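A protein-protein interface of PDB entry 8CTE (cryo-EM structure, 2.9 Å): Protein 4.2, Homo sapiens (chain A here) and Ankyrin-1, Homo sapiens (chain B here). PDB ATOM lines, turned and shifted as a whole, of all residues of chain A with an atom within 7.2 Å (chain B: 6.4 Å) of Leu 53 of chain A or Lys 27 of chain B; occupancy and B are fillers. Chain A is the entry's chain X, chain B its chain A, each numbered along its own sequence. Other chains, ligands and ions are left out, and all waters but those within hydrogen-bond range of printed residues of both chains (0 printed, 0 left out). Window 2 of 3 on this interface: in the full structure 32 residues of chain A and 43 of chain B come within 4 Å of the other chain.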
ATOM      1  N   VAL A  49     -25.943  12.671 -16.147  1.00  0.00           N
ATOM      2  CA  VAL A  49     -25.941  13.681 -15.095  1.00  0.00           C
ATOM      3  C   VAL A  49     -24.872  14.715 -15.425  1.00  0.00           C
ATOM      4  O   VAL A  49     -23.695  14.374 -15.589  1.00  0.00           O
ATOM      5  CB  VAL A  49     -25.695  13.050 -13.717  1.00  0.00           C
ATOM      6  CG1 VAL A  49     -25.767  14.110 -12.629  1.00  0.00           C
ATOM      7  CG2 VAL A  49     -26.703  11.944 -13.456  1.00  0.00           C
ATOM      8  N   ARG A  50     -25.279  15.980 -15.519  1.00  0.00           N
ATOM      9  CA  ARG A  50     -24.368  17.050 -15.905  1.00  0.00           C
ATOM     10  C   ARG A  50     -23.431  17.424 -14.764  1.00  0.00           C
ATOM     11  O   ARG A  50     -22.209  17.303 -14.891  1.00  0.00           O
ATOM     12  CB  ARG A  50     -25.158  18.277 -16.365  1.00  0.00           C
ATOM     13  N   ALA A  51     -23.993  17.879 -13.649  1.00  0.00           N
ATOM     14  CA  ALA A  51     -23.223  18.292 -12.483  1.00  0.00           C
ATOM     15  C   ALA A  51     -23.496  17.316 -11.346  1.00  0.00           C
ATOM     16  O   ALA A  51     -24.656  17.079 -10.992  1.00  0.00           O
ATOM     17  CB  ALA A  51     -23.576  19.720 -12.071  1.00  0.00           C
ATOM     18  N   PHE A  52     -22.427  16.756 -10.775  1.00  0.00           N
ATOM     19  CA  PHE A  52     -22.592  15.709  -9.772  1.00  0.00           C
ATOM     20  C   PHE A  52     -23.055  16.272  -8.433  1.00  0.00           C
ATOM     21  O   PHE A  52     -23.918  15.682  -7.776  1.00  0.00           O
ATOM     22  CB  PHE A  52     -21.288  14.933  -9.598  1.00  0.00           C
ATOM     23  CG  PHE A  52     -21.311  13.965  -8.448  1.00  0.00           C
ATOM     24  CD1 PHE A  52     -22.131  12.849  -8.483  1.00  0.00           C
ATOM     25  CD2 PHE A  52     -20.515  14.171  -7.334  1.00  0.00           C
ATOM     26  CE1 PHE A  52     -22.159  11.957  -7.426  1.00  0.00           C
ATOM     27  CE2 PHE A  52     -20.537  13.281  -6.274  1.00  0.00           C
ATOM     28  CZ  PHE A  52     -21.360  12.172  -6.322  1.00  0.00           C
ATOM     29  N   LEU A  53     -22.478  17.393  -7.999  1.00  0.00           N
ATOM     30  CA  LEU A  53     -22.779  17.908  -6.664  1.00  0.00           C
ATOM     31  C   LEU A  53     -24.222  18.387  -6.483  1.00  0.00           C
ATOM     32  O   LEU A  53     -24.829  18.026  -5.458  1.00  0.00           O
ATOM     33  CB  LEU A  53     -21.778  19.014  -6.300  1.00  0.00           C
ATOM     34  CG  LEU A  53     -20.311  18.588  -6.219  1.00  0.00           C
ATOM     35  CD1 LEU A  53     -19.423  19.781  -5.908  1.00  0.00           C
ATOM     36  CD2 LEU A  53     -20.128  17.494  -5.179  1.00  0.00           C
ATOM     37  N   PRO A  54     -24.825  19.203  -7.386  1.00  0.00           N
ATOM     38  CA  PRO A  54     -26.236  19.572  -7.189  1.00  0.00           C
ATOM     39  C   PRO A  54     -27.173  18.374  -7.221  1.00  0.00           C
ATOM     40  O   PRO A  54     -28.110  18.290  -6.421  1.00  0.00           O
ATOM     41  CB  PRO A  54     -26.516  20.533  -8.352  1.00  0.00           C
ATOM     42  CG  PRO A  54     -25.189  21.078  -8.713  1.00  0.00           C
ATOM     43  CD  PRO A  54     -24.245  19.935  -8.528  1.00  0.00           C
ATOM     44  N   ALA A  55     -26.919  17.437  -8.138  1.00  0.00           N
ATOM     45  CA  ALA A  55     -27.735  16.230  -8.213  1.00  0.00           C
ATOM     46  C   ALA A  55     -27.600  15.399  -6.945  1.00  0.00           C
ATOM     47  O   ALA A  55     -28.574  14.794  -6.479  1.00  0.00           O
ATOM     48  CB  ALA A  55     -27.343  15.405  -9.439  1.00  0.00           C
ATOM     49  N   LEU A  56     -26.392  15.349  -6.381  1.00  0.00           N
ATOM     50  CA  LEU A  56     -26.179  14.672  -5.108  1.00  0.00           C
ATOM     51  C   LEU A  56     -26.952  15.360  -3.991  1.00  0.00           C
ATOM     52  O   LEU A  56     -27.504  14.697  -3.106  1.00  0.00           O
ATOM     53  CB  LEU A  56     -24.684  14.633  -4.790  1.00  0.00           C
ATOM     54  CG  LEU A  56     -24.206  13.654  -3.718  1.00  0.00           C
ATOM     55  CD1 LEU A  56     -24.420  12.221  -4.176  1.00  0.00           C
ATOM     56  CD2 LEU A  56     -22.746  13.900  -3.370  1.00  0.00           C
ATOM     57  N   LYS A  57     -26.994  16.693  -4.012  1.00  0.00           N
ATOM     58  CA  LYS A  57     -27.790  17.426  -3.034  1.00  0.00           C
ATOM     59  C   LYS A  57     -29.290  17.244  -3.246  1.00  0.00           C
ATOM     60  O   LYS A  57     -30.064  17.452  -2.306  1.00  0.00           O
ATOM     61  CB  LYS A  57     -27.445  18.916  -3.076  1.00  0.00           C
ATOM     62  CG  LYS A  57     -26.041  19.250  -2.606  1.00  0.00           C
ATOM     63  CD  LYS A  57     -25.812  20.752  -2.602  1.00  0.00           C
ATOM     64  CE  LYS A  57     -24.430  21.102  -2.076  1.00  0.00           C
ATOM     65  NZ  LYS A  57     -24.201  22.574  -2.044  1.00  0.00           N
ATOM     66  N   LYS A  58     -29.715  16.867  -4.453  1.00  0.00           N
ATOM     67  CA  LYS A  58     -31.136  16.741  -4.757  1.00  0.00           C
ATOM     68  C   LYS A  58     -31.729  15.388  -4.381  1.00  0.00           C
ATOM     69  O   LYS A  58     -32.957  15.246  -4.414  1.00  0.00           O
ATOM     70  CB  LYS A  58     -31.382  16.987  -6.250  1.00  0.00           C
ATOM     71  CG  LYS A  58     -31.295  18.441  -6.681  1.00  0.00           C
ATOM     72  CD  LYS A  58     -31.387  18.562  -8.196  1.00  0.00           C
ATOM     73  CE  LYS A  58     -31.188  19.998  -8.655  1.00  0.00           C
ATOM     74  NZ  LYS A  58     -32.219  20.912  -8.090  1.00  0.00           N
ATOM     75  N   SER A  83     -20.865  11.916   1.788  1.00  0.00           N
ATOM     76  CA  SER A  83     -19.736  11.343   2.505  1.00  0.00           C
ATOM     77  C   SER A  83     -19.669  11.789   3.959  1.00  0.00           C
ATOM     78  O   SER A  83     -18.824  11.284   4.706  1.00  0.00           O
ATOM     79  CB  SER A  83     -18.431  11.702   1.791  1.00  0.00           C
ATOM     80  OG  SER A  83     -18.371  13.090   1.516  1.00  0.00           O
ATOM     81  N   ARG A  97     -18.645   6.727  -9.687  1.00  0.00           N
ATOM     82  CA  ARG A  97     -19.695   7.394 -10.438  1.00  0.00           C
ATOM     83  C   ARG A  97     -19.304   7.515 -11.903  1.00  0.00           C
ATOM     84  O   ARG A  97     -18.126   7.641 -12.244  1.00  0.00           O
ATOM     85  CB  ARG A  97     -19.995   8.781  -9.858  1.00  0.00           C
ATOM     86  CG  ARG A  97     -18.769   9.653  -9.673  1.00  0.00           C
ATOM     87  CD  ARG A  97     -19.087  10.850  -8.799  1.00  0.00           C
ATOM     88  NE  ARG A  97     -17.932  11.717  -8.606  1.00  0.00           N
ATOM     89  CZ  ARG A  97     -17.675  12.795  -9.334  1.00  0.00           C
ATOM     90  NH1 ARG A  97     -18.471  13.168 -10.322  1.00  0.00           N
ATOM     91  NH2 ARG A  97     -16.591  13.516  -9.062  1.00  0.00           N
ATOM     92  N   TRP A 102     -24.360   5.601 -10.672  1.00  0.00           N
ATOM     93  CA  TRP A 102     -23.747   5.867  -9.378  1.00  0.00           C
ATOM     94  C   TRP A 102     -23.598   4.558  -8.615  1.00  0.00           C
ATOM     95  O   TRP A 102     -24.575   3.823  -8.442  1.00  0.00           O
ATOM     96  CB  TRP A 102     -24.586   6.847  -8.554  1.00  0.00           C
ATOM     97  CG  TRP A 102     -24.523   8.267  -9.016  1.00  0.00           C
ATOM     98  CD1 TRP A 102     -23.762   8.770 -10.030  1.00  0.00           C
ATOM     99  CD2 TRP A 102     -25.250   9.375  -8.473  1.00  0.00           C
ATOM    100  NE1 TRP A 102     -23.973  10.121 -10.155  1.00  0.00           N
ATOM    101  CE2 TRP A 102     -24.883  10.517  -9.210  1.00  0.00           C
ATOM    102  CE3 TRP A 102     -26.180   9.510  -7.436  1.00  0.00           C
ATOM    103  CZ2 TRP A 102     -25.412  11.779  -8.943  1.00  0.00           C
ATOM    104  CZ3 TRP A 102     -26.702  10.763  -7.172  1.00  0.00           C
ATOM    105  CH2 TRP A 102     -26.316  11.880  -7.922  1.00  0.00           C
ATOM    106  N   ALA B  12      -9.011  25.602  -8.907  1.00  0.00           N
ATOM    107  CA  ALA B  12      -9.552  24.351  -8.386  1.00  0.00           C
ATOM    108  C   ALA B  12      -8.931  24.002  -7.040  1.00  0.00           C
ATOM    109  O   ALA B  12      -9.617  23.495  -6.144  1.00  0.00           O
ATOM    110  CB  ALA B  12      -9.325  23.222  -9.392  1.00  0.00           C
ATOM    111  N   SER B  15     -10.603  26.099  -4.454  1.00  0.00           N
ATOM    112  CA  SER B  15     -11.909  25.543  -4.116  1.00  0.00           C
ATOM    113  C   SER B  15     -11.772  24.318  -3.220  1.00  0.00           C
ATOM    114  O   SER B  15     -12.568  24.127  -2.293  1.00  0.00           O
ATOM    115  CB  SER B  15     -12.678  25.194  -5.390  1.00  0.00           C
ATOM    116  OG  SER B  15     -12.886  26.343  -6.193  1.00  0.00           O
ATOM    117  N   PHE B  16     -10.770  23.477  -3.483  1.00  0.00           N
ATOM    118  CA  PHE B  16     -10.530  22.314  -2.631  1.00  0.00           C
ATOM    119  C   PHE B  16     -10.156  22.731  -1.214  1.00  0.00           C
ATOM    120  O   PHE B  16     -10.640  22.144  -0.239  1.00  0.00           O
ATOM    121  CB  PHE B  16      -9.436  21.438  -3.243  1.00  0.00           C
ATOM    122  CG  PHE B  16      -8.874  20.415  -2.296  1.00  0.00           C
ATOM    123  CD1 PHE B  16      -9.610  19.295  -1.947  1.00  0.00           C
ATOM    124  CD2 PHE B  16      -7.603  20.567  -1.765  1.00  0.00           C
ATOM    125  CE1 PHE B  16      -9.091  18.350  -1.078  1.00  0.00           C
ATOM    126  CE2 PHE B  16      -7.080  19.627  -0.896  1.00  0.00           C
ATOM    127  CZ  PHE B  16      -7.826  18.516  -0.553  1.00  0.00           C
ATOM    128  N   ARG B  18     -10.953  25.586   0.245  1.00  0.00           N
ATOM    129  CA  ARG B  18     -12.147  26.161   0.860  1.00  0.00           C
ATOM    130  C   ARG B  18     -13.120  25.076   1.305  1.00  0.00           C
ATOM    131  O   ARG B  18     -13.747  25.191   2.364  1.00  0.00           O
ATOM    132  CB  ARG B  18     -12.821  27.131  -0.110  1.00  0.00           C
ATOM    133  CG  ARG B  18     -12.068  28.439  -0.290  1.00  0.00           C
ATOM    134  CD  ARG B  18     -12.748  29.349  -1.299  1.00  0.00           C
ATOM    135  NE  ARG B  18     -12.753  28.771  -2.638  1.00  0.00           N
ATOM    136  CZ  ARG B  18     -13.208  29.390  -3.719  1.00  0.00           C
ATOM    137  NH1 ARG B  18     -13.705  30.614  -3.657  1.00  0.00           N
ATOM    138  NH2 ARG B  18     -13.163  28.764  -4.892  1.00  0.00           N
ATOM    139  N   ALA B  19     -13.265  24.017   0.504  1.00  0.00           N
ATOM    140  CA  ALA B  19     -14.114  22.897   0.899  1.00  0.00           C
ATOM    141  C   ALA B  19     -13.554  22.183   2.123  1.00  0.00           C
ATOM    142  O   ALA B  19     -14.312  21.752   3.000  1.00  0.00           O
ATOM    143  CB  ALA B  19     -14.272  21.921  -0.267  1.00  0.00           C
ATOM    144  N   ASN B  24     -16.931  20.683   3.575  1.00  0.00           N
ATOM    145  CA  ASN B  24     -17.628  20.105   2.427  1.00  0.00           C
ATOM    146  C   ASN B  24     -16.772  18.966   1.889  1.00  0.00           C
ATOM    147  O   ASN B  24     -15.900  19.157   1.040  1.00  0.00           O
ATOM    148  CB  ASN B  24     -17.893  21.167   1.366  1.00  0.00           C
ATOM    149  CG  ASN B  24     -18.984  20.762   0.391  1.00  0.00           C
ATOM    150  OD1 ASN B  24     -19.135  19.587   0.060  1.00  0.00           O
ATOM    151  ND2 ASN B  24     -19.752  21.740  -0.073  1.00  0.00           N
ATOM    152  N   LEU B  25     -17.026  17.759   2.401  1.00  0.00           N
ATOM    153  CA  LEU B  25     -16.208  16.608   2.035  1.00  0.00           C
ATOM    154  C   LEU B  25     -16.474  16.165   0.602  1.00  0.00           C
ATOM    155  O   LEU B  25     -15.558  15.708  -0.093  1.00  0.00           O
ATOM    156  CB  LEU B  25     -16.459  15.462   3.014  1.00  0.00           C
ATOM    157  CG  LEU B  25     -15.626  14.189   2.871  1.00  0.00           C
ATOM    158  CD1 LEU B  25     -14.147  14.510   2.816  1.00  0.00           C
ATOM    159  CD2 LEU B  25     -15.926  13.245   4.021  1.00  0.00           C
ATOM    160  N   ASP B  26     -17.723  16.286   0.143  1.00  0.00           N
ATOM    161  CA  ASP B  26     -18.063  15.862  -1.213  1.00  0.00           C
ATOM    162  C   ASP B  26     -17.324  16.689  -2.258  1.00  0.00           C
ATOM    163  O   ASP B  26     -16.810  16.142  -3.241  1.00  0.00           O
ATOM    164  CB  ASP B  26     -19.574  15.954  -1.428  1.00  0.00           C
ATOM    165  CG  ASP B  26     -20.348  14.998  -0.544  1.00  0.00           C
ATOM    166  OD1 ASP B  26     -19.837  13.892  -0.269  1.00  0.00           O
ATOM    167  OD2 ASP B  26     -21.470  15.353  -0.124  1.00  0.00           O
ATOM    168  N   LYS B  27     -17.260  18.008  -2.063  1.00  0.00           N
ATOM    169  CA  LYS B  27     -16.558  18.867  -3.013  1.00  0.00           C
ATOM    170  C   LYS B  27     -15.063  18.568  -3.024  1.00  0.00           C
ATOM    171  O   LYS B  27     -14.433  18.554  -4.089  1.00  0.00           O
ATOM    172  CB  LYS B  27     -16.816  20.335  -2.678  1.00  0.00           C
ATOM    173  CG  LYS B  27     -16.603  21.293  -3.840  1.00  0.00           C
ATOM    174  CD  LYS B  27     -17.075  22.695  -3.486  1.00  0.00           C
ATOM    175  CE  LYS B  27     -17.105  23.601  -4.708  1.00  0.00           C
ATOM    176  NZ  LYS B  27     -15.759  23.764  -5.318  1.00  0.00           N
ATOM    177  N   ALA B  28     -14.478  18.325  -1.849  1.00  0.00           N
ATOM    178  CA  ALA B  28     -13.062  17.982  -1.778  1.00  0.00           C
ATOM    179  C   ALA B  28     -12.776  16.659  -2.477  1.00  0.00           C
ATOM    180  O   ALA B  28     -11.779  16.530  -3.199  1.00  0.00           O
ATOM    181  CB  ALA B  28     -12.607  17.931  -0.320  1.00  0.00           C
ATOM    182  N   LEU B  29     -13.642  15.660  -2.276  1.00  0.00           N
ATOM    183  CA  LEU B  29     -13.465  14.381  -2.957  1.00  0.00           C
ATOM    184  C   LEU B  29     -13.622  14.529  -4.465  1.00  0.00           C
ATOM    185  O   LEU B  29     -12.894  13.895  -5.236  1.00  0.00           O
ATOM    186  CB  LEU B  29     -14.454  13.351  -2.408  1.00  0.00           C
ATOM    187  CG  LEU B  29     -14.197  12.867  -0.979  1.00  0.00           C
ATOM    188  CD1 LEU B  29     -15.255  11.868  -0.544  1.00  0.00           C
ATOM    189  CD2 LEU B  29     -12.807  12.266  -0.858  1.00  0.00           C
ATOM    190  N   ASP B  30     -14.568  15.364  -4.905  1.00  0.00           N
ATOM    191  CA  ASP B  30     -14.733  15.617  -6.334  1.00  0.00           C
ATOM    192  C   ASP B  30     -13.494  16.284  -6.921  1.00  0.00           C
ATOM    193  O   ASP B  30     -13.055  15.935  -8.024  1.00  0.00           O
ATOM    194  CB  ASP B  30     -15.978  16.476  -6.570  1.00  0.00           C
ATOM    195  CG  ASP B  30     -16.399  16.518  -8.030  1.00  0.00           C
ATOM    196  OD1 ASP B  30     -15.623  17.013  -8.875  1.00  0.00           O
ATOM    197  OD2 ASP B  30     -17.516  16.050  -8.335  1.00  0.00           O
ATOM    198  N   HIS B  31     -12.919  17.250  -6.199  1.00  0.00           N
ATOM    199  CA  HIS B  31     -11.704  17.905  -6.675  1.00  0.00           C
ATOM    200  C   HIS B  31     -10.535  16.929  -6.735  1.00  0.00           C
ATOM    201  O   HIS B  31      -9.740  16.965  -7.681  1.00  0.00           O
ATOM    202  CB  HIS B  31     -11.365  19.099  -5.786  1.00  0.00           C
ATOM    203  CG  HIS B  31     -12.100  20.349  -6.153  1.00  0.00           C
ATOM    204  ND1 HIS B  31     -11.710  21.162  -7.196  1.00  0.00           N
ATOM    205  CD2 HIS B  31     -13.200  20.927  -5.618  1.00  0.00           C
ATOM    206  CE1 HIS B  31     -12.539  22.185  -7.287  1.00  0.00           C
ATOM    207  NE2 HIS B  31     -13.453  22.066  -6.342  1.00  0.00           N
ATOM    208  N   LEU B  32     -10.413  16.054  -5.735  1.00  0.00           N
ATOM    209  CA  LEU B  32      -9.355  15.047  -5.761  1.00  0.00           C
ATOM    210  C   LEU B  32      -9.546  14.074  -6.919  1.00  0.00           C
ATOM    211  O   LEU B  32      -8.570  13.633  -7.536  1.00  0.00           O
ATOM    212  CB  LEU B  32      -9.305  14.297  -4.430  1.00  0.00           C
ATOM    213  CG  LEU B  32      -8.789  15.092  -3.231  1.00  0.00           C
ATOM    214  CD1 LEU B  32      -8.787  14.234  -1.978  1.00  0.00           C
ATOM    215  CD2 LEU B  32      -7.401  15.638  -3.513  1.00  0.00           C
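Of the 13 printed residues of chain A, 5 touch a printed residue of chain B.
Among the printed residues, 7 pairs touch across the chains.
Among the printed residues, pairs that only touch across the chains: Phe 52 of chain A with Asp 30 of chain B, Leu 53 of chain A with Lys 27 of chain B, Leu 56 of chain A with Asp 26 of chain B, Ser 83 of chain A with Leu 25 of chain B and Ser 83 of chain A with Leu 29 of chain B.
Leu 53 of chain A touches one residue of chain B.
Printed residues of chain A within 4 Å of Lys 27 of chain B: Leu 53 (3.8 Å).
Of the printed residues of chain A, Asp 26 of chain B touches Leu 56 and Ser 83.
Of the printed residues of chain A, Asp 30 of chain B touches Phe 52 (3.7 Å) and Arg 97 (2.8 Å).
Of the printed residues of chain A, Leu 29 of chain B touches Ser 83.
Of the printed residues of chain B, Arg 97 of chain A touches Asp 30 (2.8 Å).
Printed residues of chain B within 4 Å of Ser 83 of chain A: Leu 25, Asp 26 and Leu 29.
The nearest residue of chain B that does not touch Leu 53 of chain A is Asp 26 of chain B (4.1 Å).
The nearest printed residue of chain B that does not touch Arg 97 of chain A is Leu 29 of chain B (5.3 Å).
OD1 of Asp 26 of chain B sits at hydrogen-bond distance from OG of Ser 83 of chain A, at 2.4 Å.
OD2 of Asp 30 of chain B lies within salt-bridge range of NH2 of Arg 97 of chain A, 2.8 Å away.
The side-chain amide oxygen of Asn 24 of chain B lies within hydrogen-bond range of the backbone NH of Lys 27 of chain B.
A ring nitrogen (NE2) of His 31 of chain B sits at hydrogen-bond distance from the side-chain amino group (NZ) of Lys 27 of chain B, 3.0 Å away.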
